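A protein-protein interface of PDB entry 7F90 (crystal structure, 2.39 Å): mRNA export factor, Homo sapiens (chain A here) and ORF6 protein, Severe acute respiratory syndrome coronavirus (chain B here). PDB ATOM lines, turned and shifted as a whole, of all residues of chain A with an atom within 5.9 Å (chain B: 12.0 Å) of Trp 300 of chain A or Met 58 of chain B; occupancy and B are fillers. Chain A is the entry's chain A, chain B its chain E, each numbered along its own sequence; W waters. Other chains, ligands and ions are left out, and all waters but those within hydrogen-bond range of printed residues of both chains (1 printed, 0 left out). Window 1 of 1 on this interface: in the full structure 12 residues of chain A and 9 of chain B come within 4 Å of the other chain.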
ATOM      1  N   PHE A 255      -4.596  -3.122  -0.283  1.00  0.00           N
ATOM      2  CA  PHE A 255      -3.144  -2.993  -0.276  1.00  0.00           C
ATOM      3  C   PHE A 255      -2.773  -1.571   0.129  1.00  0.00           C
ATOM      4  O   PHE A 255      -3.632  -0.692   0.260  1.00  0.00           O
ATOM      5  CB  PHE A 255      -2.547  -3.383  -1.642  1.00  0.00           C
ATOM      6  CG  PHE A 255      -2.928  -2.460  -2.771  1.00  0.00           C
ATOM      7  CD1 PHE A 255      -4.166  -2.563  -3.375  1.00  0.00           C
ATOM      8  CD2 PHE A 255      -2.035  -1.499  -3.229  1.00  0.00           C
ATOM      9  CE1 PHE A 255      -4.520  -1.717  -4.406  1.00  0.00           C
ATOM     10  CE2 PHE A 255      -2.380  -0.646  -4.265  1.00  0.00           C
ATOM     11  CZ  PHE A 255      -3.623  -0.757  -4.856  1.00  0.00           C
ATOM     12  N   PHE A 257       0.615   1.290  -0.680  1.00  0.00           N
ATOM     13  CA  PHE A 257       1.777   1.569  -1.510  1.00  0.00           C
ATOM     14  C   PHE A 257       2.513   2.781  -0.961  1.00  0.00           C
ATOM     15  O   PHE A 257       1.962   3.579  -0.199  1.00  0.00           O
ATOM     16  CB  PHE A 257       1.382   1.768  -2.988  1.00  0.00           C
ATOM     17  CG  PHE A 257       0.477   2.950  -3.238  1.00  0.00           C
ATOM     18  CD1 PHE A 257      -0.902   2.813  -3.195  1.00  0.00           C
ATOM     19  CD2 PHE A 257       1.007   4.198  -3.538  1.00  0.00           C
ATOM     20  CE1 PHE A 257      -1.731   3.902  -3.431  1.00  0.00           C
ATOM     21  CE2 PHE A 257       0.185   5.287  -3.772  1.00  0.00           C
ATOM     22  CZ  PHE A 257      -1.183   5.141  -3.721  1.00  0.00           C
ATOM     23  N   LYS A 258       3.782   2.884  -1.337  1.00  0.00           N
ATOM     24  CA  LYS A 258       4.651   3.948  -0.867  1.00  0.00           C
ATOM     25  C   LYS A 258       4.626   5.097  -1.865  1.00  0.00           C
ATOM     26  O   LYS A 258       4.413   4.902  -3.069  1.00  0.00           O
ATOM     27  CB  LYS A 258       6.076   3.432  -0.660  1.00  0.00           C
ATOM     28  CG  LYS A 258       6.174   2.383   0.448  1.00  0.00           C
ATOM     29  CD  LYS A 258       7.607   2.137   0.893  1.00  0.00           C
ATOM     30  CE  LYS A 258       8.424   1.487  -0.213  1.00  0.00           C
ATOM     31  NZ  LYS A 258       7.950   0.113  -0.557  1.00  0.00           N
ATOM     32  N   CYS A 259       4.823   6.305  -1.344  1.00  0.00           N
ATOM     33  CA  CYS A 259       4.661   7.518  -2.130  1.00  0.00           C
ATOM     34  C   CYS A 259       5.241   8.674  -1.338  1.00  0.00           C
ATOM     35  O   CYS A 259       5.351   8.619  -0.110  1.00  0.00           O
ATOM     36  CB  CYS A 259       3.192   7.780  -2.468  1.00  0.00           C
ATOM     37  SG  CYS A 259       2.113   7.836  -1.032  1.00  0.00           S
ATOM     38  N   HIS A 260       5.613   9.725  -2.067  1.00  0.00           N
ATOM     39  CA  HIS A 260       6.081  10.972  -1.466  1.00  0.00           C
ATOM     40  C   HIS A 260       7.299  10.730  -0.579  1.00  0.00           C
ATOM     41  O   HIS A 260       7.387  11.206   0.555  1.00  0.00           O
ATOM     42  CB  HIS A 260       4.952  11.651  -0.699  1.00  0.00           C
ATOM     43  CG  HIS A 260       3.810  12.067  -1.572  1.00  0.00           C
ATOM     44  ND1 HIS A 260       3.839  13.212  -2.340  1.00  0.00           N
ATOM     45  CD2 HIS A 260       2.607  11.491  -1.799  1.00  0.00           C
ATOM     46  CE1 HIS A 260       2.699  13.324  -2.999  1.00  0.00           C
ATOM     47  NE2 HIS A 260       1.934  12.293  -2.689  1.00  0.00           N
ATOM     48  N   GLY A 286     -11.568   7.724 -12.261  1.00  0.00           N
ATOM     49  CA  GLY A 286     -11.410   6.889 -11.089  1.00  0.00           C
ATOM     50  C   GLY A 286      -9.977   6.633 -10.681  1.00  0.00           C
ATOM     51  O   GLY A 286      -9.751   5.872  -9.736  1.00  0.00           O
ATOM     52  N   THR A 287      -9.006   7.194 -11.398  1.00  0.00           N
ATOM     53  CA  THR A 287      -7.633   7.276 -10.920  1.00  0.00           C
ATOM     54  C   THR A 287      -7.581   8.318  -9.808  1.00  0.00           C
ATOM     55  O   THR A 287      -8.600   8.922  -9.454  1.00  0.00           O
ATOM     56  CB  THR A 287      -6.701   7.612 -12.079  1.00  0.00           C
ATOM     57  OG1 THR A 287      -7.162   8.799 -12.737  1.00  0.00           O
ATOM     58  CG2 THR A 287      -6.700   6.457 -13.063  1.00  0.00           C
ATOM     59  N   LEU A 288      -6.391   8.550  -9.245  1.00  0.00           N
ATOM     60  CA  LEU A 288      -6.316   9.448  -8.099  1.00  0.00           C
ATOM     61  C   LEU A 288      -5.014  10.240  -8.062  1.00  0.00           C
ATOM     62  O   LEU A 288      -4.016   9.888  -8.699  1.00  0.00           O
ATOM     63  CB  LEU A 288      -6.496   8.671  -6.784  1.00  0.00           C
ATOM     64  CG  LEU A 288      -5.359   7.770  -6.292  1.00  0.00           C
ATOM     65  CD1 LEU A 288      -5.426   7.655  -4.775  1.00  0.00           C
ATOM     66  CD2 LEU A 288      -5.431   6.389  -6.924  1.00  0.00           C
ATOM     67  N   ALA A 289      -5.048  11.328  -7.289  1.00  0.00           N
ATOM     68  CA  ALA A 289      -3.899  12.194  -7.078  1.00  0.00           C
ATOM     69  C   ALA A 289      -3.591  12.236  -5.591  1.00  0.00           C
ATOM     70  O   ALA A 289      -4.510  12.185  -4.766  1.00  0.00           O
ATOM     71  CB  ALA A 289      -4.169  13.611  -7.594  1.00  0.00           C
ATOM     72  N   THR A 290      -2.306  12.302  -5.249  1.00  0.00           N
ATOM     73  CA  THR A 290      -1.868  12.575  -3.887  1.00  0.00           C
ATOM     74  C   THR A 290      -0.924  13.769  -3.900  1.00  0.00           C
ATOM     75  O   THR A 290      -0.230  14.012  -4.889  1.00  0.00           O
ATOM     76  CB  THR A 290      -1.150  11.373  -3.254  1.00  0.00           C
ATOM     77  OG1 THR A 290       0.135  11.211  -3.869  1.00  0.00           O
ATOM     78  CG2 THR A 290      -1.966  10.107  -3.433  1.00  0.00           C
ATOM     79  N   SER A 298       1.463  13.559  -7.304  1.00  0.00           N
ATOM     80  CA  SER A 298       1.591  12.324  -8.065  1.00  0.00           C
ATOM     81  C   SER A 298       0.204  11.807  -8.418  1.00  0.00           C
ATOM     82  O   SER A 298      -0.757  11.996  -7.665  1.00  0.00           O
ATOM     83  CB  SER A 298       2.370  11.255  -7.286  1.00  0.00           C
ATOM     84  OG  SER A 298       3.749  11.572  -7.179  1.00  0.00           O
ATOM     85  N   PHE A 299       0.120  11.152  -9.574  1.00  0.00           N
ATOM     86  CA  PHE A 299      -1.105  10.548 -10.071  1.00  0.00           C
ATOM     87  C   PHE A 299      -0.963   9.034 -10.028  1.00  0.00           C
ATOM     88  O   PHE A 299       0.140   8.496 -10.155  1.00  0.00           O
ATOM     89  CB  PHE A 299      -1.402  11.022 -11.490  1.00  0.00           C
ATOM     90  CG  PHE A 299      -1.643  12.505 -11.591  1.00  0.00           C
ATOM     91  CD1 PHE A 299      -2.020  13.245 -10.474  1.00  0.00           C
ATOM     92  CD2 PHE A 299      -1.486  13.169 -12.798  1.00  0.00           C
ATOM     93  CE1 PHE A 299      -2.243  14.616 -10.554  1.00  0.00           C
ATOM     94  CE2 PHE A 299      -1.713  14.542 -12.884  1.00  0.00           C
ATOM     95  CZ  PHE A 299      -2.092  15.267 -11.755  1.00  0.00           C
ATOM     96  N   TRP A 300      -2.091   8.351  -9.845  1.00  0.00           N
ATOM     97  CA  TRP A 300      -2.074   6.924  -9.564  1.00  0.00           C
ATOM     98  C   TRP A 300      -3.285   6.245 -10.186  1.00  0.00           C
ATOM     99  O   TRP A 300      -4.342   6.859 -10.356  1.00  0.00           O
ATOM    100  CB  TRP A 300      -2.066   6.664  -8.053  1.00  0.00           C
ATOM    101  CG  TRP A 300      -1.010   7.418  -7.318  1.00  0.00           C
ATOM    102  CD1 TRP A 300      -1.112   8.676  -6.789  1.00  0.00           C
ATOM    103  CD2 TRP A 300       0.318   6.971  -7.040  1.00  0.00           C
ATOM    104  NE1 TRP A 300       0.071   9.034  -6.195  1.00  0.00           N
ATOM    105  CE2 TRP A 300       0.968   8.005  -6.335  1.00  0.00           C
ATOM    106  CE3 TRP A 300       1.023   5.795  -7.315  1.00  0.00           C
ATOM    107  CZ2 TRP A 300       2.290   7.897  -5.903  1.00  0.00           C
ATOM    108  CZ3 TRP A 300       2.334   5.689  -6.884  1.00  0.00           C
ATOM    109  CH2 TRP A 300       2.957   6.735  -6.189  1.00  0.00           C
ATOM    110  N   ASP A 301      -3.107   4.959 -10.510  1.00  0.00           N
ATOM    111  CA  ASP A 301      -4.171   4.057 -10.945  1.00  0.00           C
ATOM    112  C   ASP A 301      -4.216   2.894  -9.956  1.00  0.00           C
ATOM    113  O   ASP A 301      -3.307   2.060  -9.928  1.00  0.00           O
ATOM    114  CB  ASP A 301      -3.917   3.564 -12.369  1.00  0.00           C
ATOM    115  CG  ASP A 301      -5.017   2.652 -12.886  1.00  0.00           C
ATOM    116  OD1 ASP A 301      -5.624   1.925 -12.077  1.00  0.00           O
ATOM    117  OD2 ASP A 301      -5.266   2.661 -14.113  1.00  0.00           O
ATOM    118  N   LYS A 302      -5.261   2.834  -9.134  1.00  0.00           N
ATOM    119  CA  LYS A 302      -5.312   1.799  -8.107  1.00  0.00           C
ATOM    120  C   LYS A 302      -5.754   0.446  -8.649  1.00  0.00           C
ATOM    121  O   LYS A 302      -5.519  -0.575  -7.994  1.00  0.00           O
ATOM    122  CB  LYS A 302      -6.233   2.235  -6.963  1.00  0.00           C
ATOM    123  CG  LYS A 302      -7.642   2.670  -7.367  1.00  0.00           C
ATOM    124  CD  LYS A 302      -8.624   1.501  -7.386  1.00  0.00           C
ATOM    125  CE  LYS A 302     -10.053   2.007  -7.497  1.00  0.00           C
ATOM    126  NZ  LYS A 302     -11.061   0.923  -7.548  1.00  0.00           N
ATOM    127  N   ARG A 305      -2.516  -0.549 -10.403  1.00  0.00           N
ATOM    128  CA  ARG A 305      -1.468  -0.502  -9.382  1.00  0.00           C
ATOM    129  C   ARG A 305      -0.181   0.096  -9.945  1.00  0.00           C
ATOM    130  O   ARG A 305       0.903  -0.474  -9.816  1.00  0.00           O
ATOM    131  CB  ARG A 305      -1.212  -1.886  -8.784  1.00  0.00           C
ATOM    132  CG  ARG A 305      -2.427  -2.453  -8.100  1.00  0.00           C
ATOM    133  CD  ARG A 305      -2.097  -3.605  -7.173  1.00  0.00           C
ATOM    134  NE  ARG A 305      -3.320  -4.220  -6.674  1.00  0.00           N
ATOM    135  CZ  ARG A 305      -3.365  -5.199  -5.776  1.00  0.00           C
ATOM    136  NH1 ARG A 305      -2.246  -5.681  -5.263  1.00  0.00           N
ATOM    137  NH2 ARG A 305      -4.534  -5.696  -5.388  1.00  0.00           N
ATOM    138  N   THR A 306      -0.310   1.269 -10.555  1.00  0.00           N
ATOM    139  CA  THR A 306       0.796   1.943 -11.213  1.00  0.00           C
ATOM    140  C   THR A 306       0.841   3.401 -10.789  1.00  0.00           C
ATOM    141  O   THR A 306      -0.158   3.971 -10.342  1.00  0.00           O
ATOM    142  CB  THR A 306       0.673   1.861 -12.742  1.00  0.00           C
ATOM    143  OG1 THR A 306      -0.641   2.269 -13.138  1.00  0.00           O
ATOM    144  CG2 THR A 306       0.956   0.443 -13.215  1.00  0.00           C
ATOM    145  N   LYS A 307       2.019   3.999 -10.936  1.00  0.00           N
ATOM    146  CA  LYS A 307       2.182   5.435 -10.761  1.00  0.00           C
ATOM    147  C   LYS A 307       2.142   6.073 -12.141  1.00  0.00           C
ATOM    148  O   LYS A 307       2.976   5.763 -12.999  1.00  0.00           O
ATOM    149  CB  LYS A 307       3.488   5.778 -10.047  1.00  0.00           C
ATOM    150  CG  LYS A 307       3.561   7.243  -9.613  1.00  0.00           C
ATOM    151  CD  LYS A 307       4.859   7.567  -8.890  1.00  0.00           C
ATOM    152  CE  LYS A 307       6.033   7.600  -9.850  1.00  0.00           C
ATOM    153  NZ  LYS A 307       7.095   8.525  -9.370  1.00  0.00           N
ATOM    154  N   LEU A 308       1.165   6.945 -12.364  1.00  0.00           N
ATOM    155  CA  LEU A 308       0.997   7.525 -13.689  1.00  0.00           C
ATOM    156  C   LEU A 308       1.903   8.727 -13.911  1.00  0.00           C
ATOM    157  O   LEU A 308       2.337   8.964 -15.043  1.00  0.00           O
ATOM    158  CB  LEU A 308      -0.459   7.934 -13.910  1.00  0.00           C
ATOM    159  CG  LEU A 308      -1.491   6.805 -13.978  1.00  0.00           C
ATOM    160  CD1 LEU A 308      -2.864   7.368 -14.322  1.00  0.00           C
ATOM    161  CD2 LEU A 308      -1.065   5.752 -14.986  1.00  0.00           C
ATOM    162  N   LYS A 309       2.205   9.490 -12.865  1.00  0.00           N
ATOM    163  CA  LYS A 309       2.975  10.716 -13.035  1.00  0.00           C
ATOM    164  C   LYS A 309       3.430  11.218 -11.676  1.00  0.00           C
ATOM    165  O   LYS A 309       2.736  11.045 -10.673  1.00  0.00           O
ATOM    166  CB  LYS A 309       2.150  11.795 -13.747  1.00  0.00           C
ATOM    167  CG  LYS A 309       2.877  13.112 -13.981  1.00  0.00           C
ATOM    168  CD  LYS A 309       2.043  14.025 -14.875  1.00  0.00           C
ATOM    169  CE  LYS A 309       2.606  15.435 -14.948  1.00  0.00           C
ATOM    170  NZ  LYS A 309       2.477  16.145 -13.646  1.00  0.00           N
ATOM    171  N   THR A 310       4.610  11.832 -11.658  1.00  0.00           N
ATOM    172  CA  THR A 310       5.130  12.504 -10.474  1.00  0.00           C
ATOM    173  C   THR A 310       5.751  13.812 -10.921  1.00  0.00           C
ATOM    174  O   THR A 310       6.737  13.806 -11.664  1.00  0.00           O
ATOM    175  CB  THR A 310       6.165  11.650  -9.746  1.00  0.00           C
ATOM    176  OG1 THR A 310       5.576  10.392  -9.398  1.00  0.00           O
ATOM    177  CG2 THR A 310       6.638  12.346  -8.468  1.00  0.00           C
ATOM    178  N   LEU A 362      -4.326  11.741 -16.263  1.00  0.00           N
ATOM    179  CA  LEU A 362      -4.888  10.815 -15.287  1.00  0.00           C
ATOM    180  C   LEU A 362      -5.764   9.734 -15.909  1.00  0.00           C
ATOM    181  O   LEU A 362      -6.326   8.918 -15.170  1.00  0.00           O
ATOM    182  CB  LEU A 362      -5.700  11.582 -14.240  1.00  0.00           C
ATOM    183  CG  LEU A 362      -4.876  12.256 -13.139  1.00  0.00           C
ATOM    184  CD1 LEU A 362      -5.368  13.685 -12.909  1.00  0.00           C
ATOM    185  CD2 LEU A 362      -4.945  11.450 -11.864  1.00  0.00           C
ATOM    186  N   ASP B  53       7.418  11.261 -16.441  1.00  0.00           N
ATOM    187  CA  ASP B  53       5.989  10.986 -16.476  1.00  0.00           C
ATOM    188  C   ASP B  53       5.703   9.594 -17.026  1.00  0.00           C
ATOM    189  O   ASP B  53       4.562   9.281 -17.367  1.00  0.00           O
ATOM    190  CB  ASP B  53       5.266  12.035 -17.322  1.00  0.00           C
ATOM    191  CG  ASP B  53       6.011  13.357 -17.373  1.00  0.00           C
ATOM    192  OD1 ASP B  53       7.036  13.431 -18.082  1.00  0.00           O
ATOM    193  OD2 ASP B  53       5.582  14.324 -16.708  1.00  0.00           O
ATOM    194  N   ASP B  54       6.739   8.767 -17.128  1.00  0.00           N
ATOM    195  CA  ASP B  54       6.547   7.388 -17.551  1.00  0.00           C
ATOM    196  C   ASP B  54       5.765   6.620 -16.492  1.00  0.00           C
ATOM    197  O   ASP B  54       5.934   6.841 -15.291  1.00  0.00           O
ATOM    198  CB  ASP B  54       7.896   6.710 -17.800  1.00  0.00           C
ATOM    199  CG  ASP B  54       8.603   7.243 -19.034  1.00  0.00           C
ATOM    200  OD1 ASP B  54       7.945   7.891 -19.875  1.00  0.00           O
ATOM    201  OD2 ASP B  54       9.822   7.003 -19.164  1.00  0.00           O
ATOM    202  N   GLU B  55       4.911   5.709 -16.947  1.00  0.00           N
ATOM    203  CA  GLU B  55       4.043   4.928 -16.071  1.00  0.00           C
ATOM    204  C   GLU B  55       4.796   3.707 -15.551  1.00  0.00           C
ATOM    205  O   GLU B  55       5.153   2.806 -16.317  1.00  0.00           O
ATOM    206  CB  GLU B  55       2.774   4.549 -16.830  1.00  0.00           C
ATOM    207  CG  GLU B  55       2.241   3.162 -16.602  1.00  0.00           C
ATOM    208  CD  GLU B  55       0.777   3.047 -17.000  1.00  0.00           C
ATOM    209  OE1 GLU B  55       0.368   3.617 -18.039  1.00  0.00           O
ATOM    210  OE2 GLU B  55       0.024   2.390 -16.256  1.00  0.00           O
ATOM    211  N   GLU B  56       5.027   3.679 -14.248  1.00  0.00           N
ATOM    212  CA  GLU B  56       5.733   2.617 -13.556  1.00  0.00           C
ATOM    213  C   GLU B  56       4.763   1.827 -12.689  1.00  0.00           C
ATOM    214  O   GLU B  56       3.614   2.227 -12.501  1.00  0.00           O
ATOM    215  CB  GLU B  56       6.841   3.192 -12.669  1.00  0.00           C
ATOM    216  CG  GLU B  56       7.547   4.428 -13.197  1.00  0.00           C
ATOM    217  CD  GLU B  56       8.460   5.052 -12.146  1.00  0.00           C
ATOM    218  OE1 GLU B  56       8.224   6.218 -11.759  1.00  0.00           O
ATOM    219  OE2 GLU B  56       9.407   4.369 -11.697  1.00  0.00           O
ATOM    220  N   PRO B  57       5.196   0.690 -12.150  1.00  0.00           N
ATOM    221  CA  PRO B  57       4.380   0.006 -11.139  1.00  0.00           C
ATOM    222  C   PRO B  57       4.581   0.589  -9.749  1.00  0.00           C
ATOM    223  O   PRO B  57       5.655   1.079  -9.393  1.00  0.00           O
ATOM    224  CB  PRO B  57       4.873  -1.448 -11.199  1.00  0.00           C
ATOM    225  CG  PRO B  57       5.699  -1.561 -12.484  1.00  0.00           C
ATOM    226  CD  PRO B  57       6.265  -0.174 -12.676  1.00  0.00           C
ATOM    227  N   MET B  58       3.520   0.526  -8.951  1.00  0.00           N
ATOM    228  CA  MET B  58       3.586   1.052  -7.596  1.00  0.00           C
ATOM    229  C   MET B  58       4.598   0.273  -6.758  1.00  0.00           C
ATOM    230  O   MET B  58       4.738  -0.945  -6.892  1.00  0.00           O
ATOM    231  CB  MET B  58       2.215   0.973  -6.919  1.00  0.00           C
ATOM    232  CG  MET B  58       1.190   2.023  -7.313  1.00  0.00           C
ATOM    233  SD  MET B  58      -0.389   1.607  -6.535  1.00  0.00           S
ATOM    234  CE  MET B  58      -1.449   2.896  -7.174  1.00  0.00           C
ATOM    235  N   GLU B  59       5.304   0.987  -5.883  1.00  0.00           N
ATOM    236  CA  GLU B  59       6.029   0.347  -4.794  1.00  0.00           C
ATOM    237  C   GLU B  59       5.029  -0.115  -3.742  1.00  0.00           C
ATOM    238  O   GLU B  59       4.660   0.658  -2.853  1.00  0.00           O
ATOM    239  CB  GLU B  59       7.038   1.305  -4.168  1.00  0.00           C
ATOM    240  CG  GLU B  59       8.476   0.994  -4.542  1.00  0.00           C
ATOM    241  CD  GLU B  59       9.423   2.151  -4.295  1.00  0.00           C
ATOM    242  OE1 GLU B  59       9.865   2.336  -3.141  1.00  0.00           O
ATOM    243  OE2 GLU B  59       9.713   2.888  -5.260  1.00  0.00           O
ATOM    244  N   LEU B  60       4.568  -1.358  -3.838  1.00  0.00           N
ATOM    245  CA  LEU B  60       3.613  -1.897  -2.876  1.00  0.00           C
ATOM    246  C   LEU B  60       4.347  -2.446  -1.660  1.00  0.00           C
ATOM    247  O   LEU B  60       5.498  -2.875  -1.750  1.00  0.00           O
ATOM    248  CB  LEU B  60       2.766  -3.005  -3.511  1.00  0.00           C
ATOM    249  CG  LEU B  60       1.913  -2.629  -4.725  1.00  0.00           C
ATOM    250  CD1 LEU B  60       1.070  -3.817  -5.175  1.00  0.00           C
ATOM    251  CD2 LEU B  60       1.035  -1.428  -4.409  1.00  0.00           C
ATOM    252  N   ASP B  61       3.679  -2.399  -0.514  1.00  0.00           N
ATOM    253  CA  ASP B  61       4.159  -3.085   0.675  1.00  0.00           C
ATOM    254  C   ASP B  61       3.791  -4.555   0.577  1.00  0.00           C
ATOM    255  O   ASP B  61       2.649  -4.895   0.257  1.00  0.00           O
ATOM    256  CB  ASP B  61       3.542  -2.477   1.923  1.00  0.00           C
ATOM    257  CG  ASP B  61       3.730  -0.999   1.984  1.00  0.00           C
ATOM    258  OD1 ASP B  61       4.866  -0.535   2.223  1.00  0.00           O
ATOM    259  OD2 ASP B  61       2.739  -0.272   1.772  1.00  0.00           O
ATOM    260  N   TYR B  62       4.752  -5.424   0.854  1.00  0.00           N
ATOM    261  CA  TYR B  62       4.531  -6.852   0.675  1.00  0.00           C
ATOM    262  C   TYR B  62       4.159  -7.548   1.976  1.00  0.00           C
ATOM    263  O   TYR B  62       3.431  -8.541   1.968  1.00  0.00           O
ATOM    264  CB  TYR B  62       5.777  -7.503   0.076  1.00  0.00           C
ATOM    265  CG  TYR B  62       6.093  -7.037  -1.324  1.00  0.00           C
ATOM    266  CD1 TYR B  62       6.887  -5.917  -1.550  1.00  0.00           C
ATOM    267  CD2 TYR B  62       5.595  -7.718  -2.422  1.00  0.00           C
ATOM    268  CE1 TYR B  62       7.172  -5.492  -2.834  1.00  0.00           C
ATOM    269  CE2 TYR B  62       5.874  -7.303  -3.704  1.00  0.00           C
ATOM    270  CZ  TYR B  62       6.662  -6.190  -3.907  1.00  0.00           C
ATOM    271  OH  TYR B  62       6.944  -5.773  -5.187  1.00  0.00           O
HETATM  272  O   HOH W   1       5.177   3.735  -5.169  1.00  0.00           O
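The side-chain carboxylate (OE2) of Glu 55 of chain B lies within hydrogen-bond range of the side-chain hydroxyl (OG1) of Thr 306 of chain A.
The backbone NH (N) of Met 58 of chain B sits at hydrogen-bond distance from the backbone carbonyl oxygen (O) of Arg 305 of chain A.
NZ of Lys 258 of chain A lies within salt-bridge range of OE1 of Glu 59 of chain B.
The side-chain carboxylate (OE1) of Glu 56 of chain B is in salt-bridge range of the side-chain amino group (NZ) of Lys 307 of chain A, 3.5 Å away.
The backbone carbonyl oxygen of Leu 308 of chain A sits close to the backbone carbonyl oxygen of Asp 53 of chain B (3.2 Å).
Phe 255 of chain A touches Met 58 of chain B.
CD1 of Phe 257 of chain A touches SD of Met 58 of chain B, at 3.6 Å.
CA of Phe 257 of chain A touches O of Glu 59 of chain B, at 3.3 Å.
Asp 61 of chain B touches Phe 257 of chain A.
O of Asp 301 of chain A touches CE of Met 58 of chain B, 3.4 Å away.
Arg 305 of chain A touches Leu 60 of chain B (CD to CD1, 3.8 Å).
Met 58 of chain B touches Thr 306 of chain A (CE to O, 3.6 Å).
Asp 54 of chain B touches Lys 307 of chain A (O to O, 3.9 Å).
CD2 of Leu 308 of chain A touches OE2 of Glu 55 of chain B, 3.8 Å away.
Asp 53 of chain B touches Lys 309 of chain A.
Water W1 lies within hydrogen-bond range of the backbone carbonyl oxygen of Lys 258 of chain A (2.5 Å) and the backbone NH of Glu 59 of chain B (2.8 Å).
Of the 22 printed residues of chain A, 10 touch a printed residue of chain B.
Among the printed residues, 22 pairs touch across the chains.
The backbone carbonyl oxygen (O) of Ser 298 of chain A lies close to the indole nitrogen (NE1) of Trp 300 of chain A.
N of Trp 300 of chain A is in hydrogen-bond range of O of Leu 288 of chain A, 2.7 Å away.
N of Asp 301 of chain A is in hydrogen-bond range of O of Thr 306 of chain A, 3.1 Å away.
The side-chain hydroxyl (OG1) of Thr 290 of chain A lies within hydrogen-bond range of the indole nitrogen (NE1) of Trp 300 of chain A (3.2 Å).
The backbone carbonyl oxygen of Phe 299 of chain A lies within hydrogen-bond range of the backbone NH of Leu 308 of chain A, at 2.9 Å.
The backbone carbonyl oxygen (O) of Lys 309 of chain A is in hydrogen-bond range of the backbone NH (N) of Phe 299 of chain A, 2.8 Å away.
Of the printed residues of chain B, Phe 255 of chain A touches Met 58 (3.8 Å) and Leu 60 (3.3 Å).
Of chain B, only Met 58 (3.6 Å), Glu 59 (3.3 Å), Leu 60 (3.5 Å) and Asp 61 (3.6 Å) come within 4 Å of Phe 257 of chain A.
No residue of chain B comes within 4 Å of Cys 259 of chain A.
No residue of chain B comes within 4 Å of Gly 286 of chain A.
Thr 287 of chain A touches none of the printed residues of chain B.
No residue of chain B comes within 4 Å of Leu 288 of chain A.
No residue of chain B comes within 4 Å of Ala 289 of chain A.
No residue of chain B comes within 4 Å of Thr 290 of chain A.
No residue of chain B comes within 4 Å of Ser 298 of chain A.
Trp 300 of chain A touches one residue of chain B.
Lys 302 of chain A touches none of the printed residues of chain B.
Thr 306 of chain A touches three residues of chain B.
Lys 307 of chain A touches just these residues of chain B: Asp 54, Glu 55 and Glu 56.
Leu 308 of chain A touches two residues of chain B.
Of the printed residues of chain B, Lys 309 of chain A touches Asp 53.
Of the printed residues of chain A, Glu 56 of chain B touches Thr 306 and Lys 307.
Of chain A, only Phe 255 (3.8 Å), Phe 257 (3.6 Å), Trp 300 (3.8 Å), Asp 301 (3.4 Å), Arg 305 (2.9 Å) and Thr 306 (3.6 Å) come within 4 Å of Met 58 of chain B.
The nearest residue of chain A that does not touch Met 58 of chain B is Lys 302 of chain A (4.1 Å).
The nearest printed residue of chain A that does not touch Leu 60 of chain B is Lys 258 of chain A (4.05 Å).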
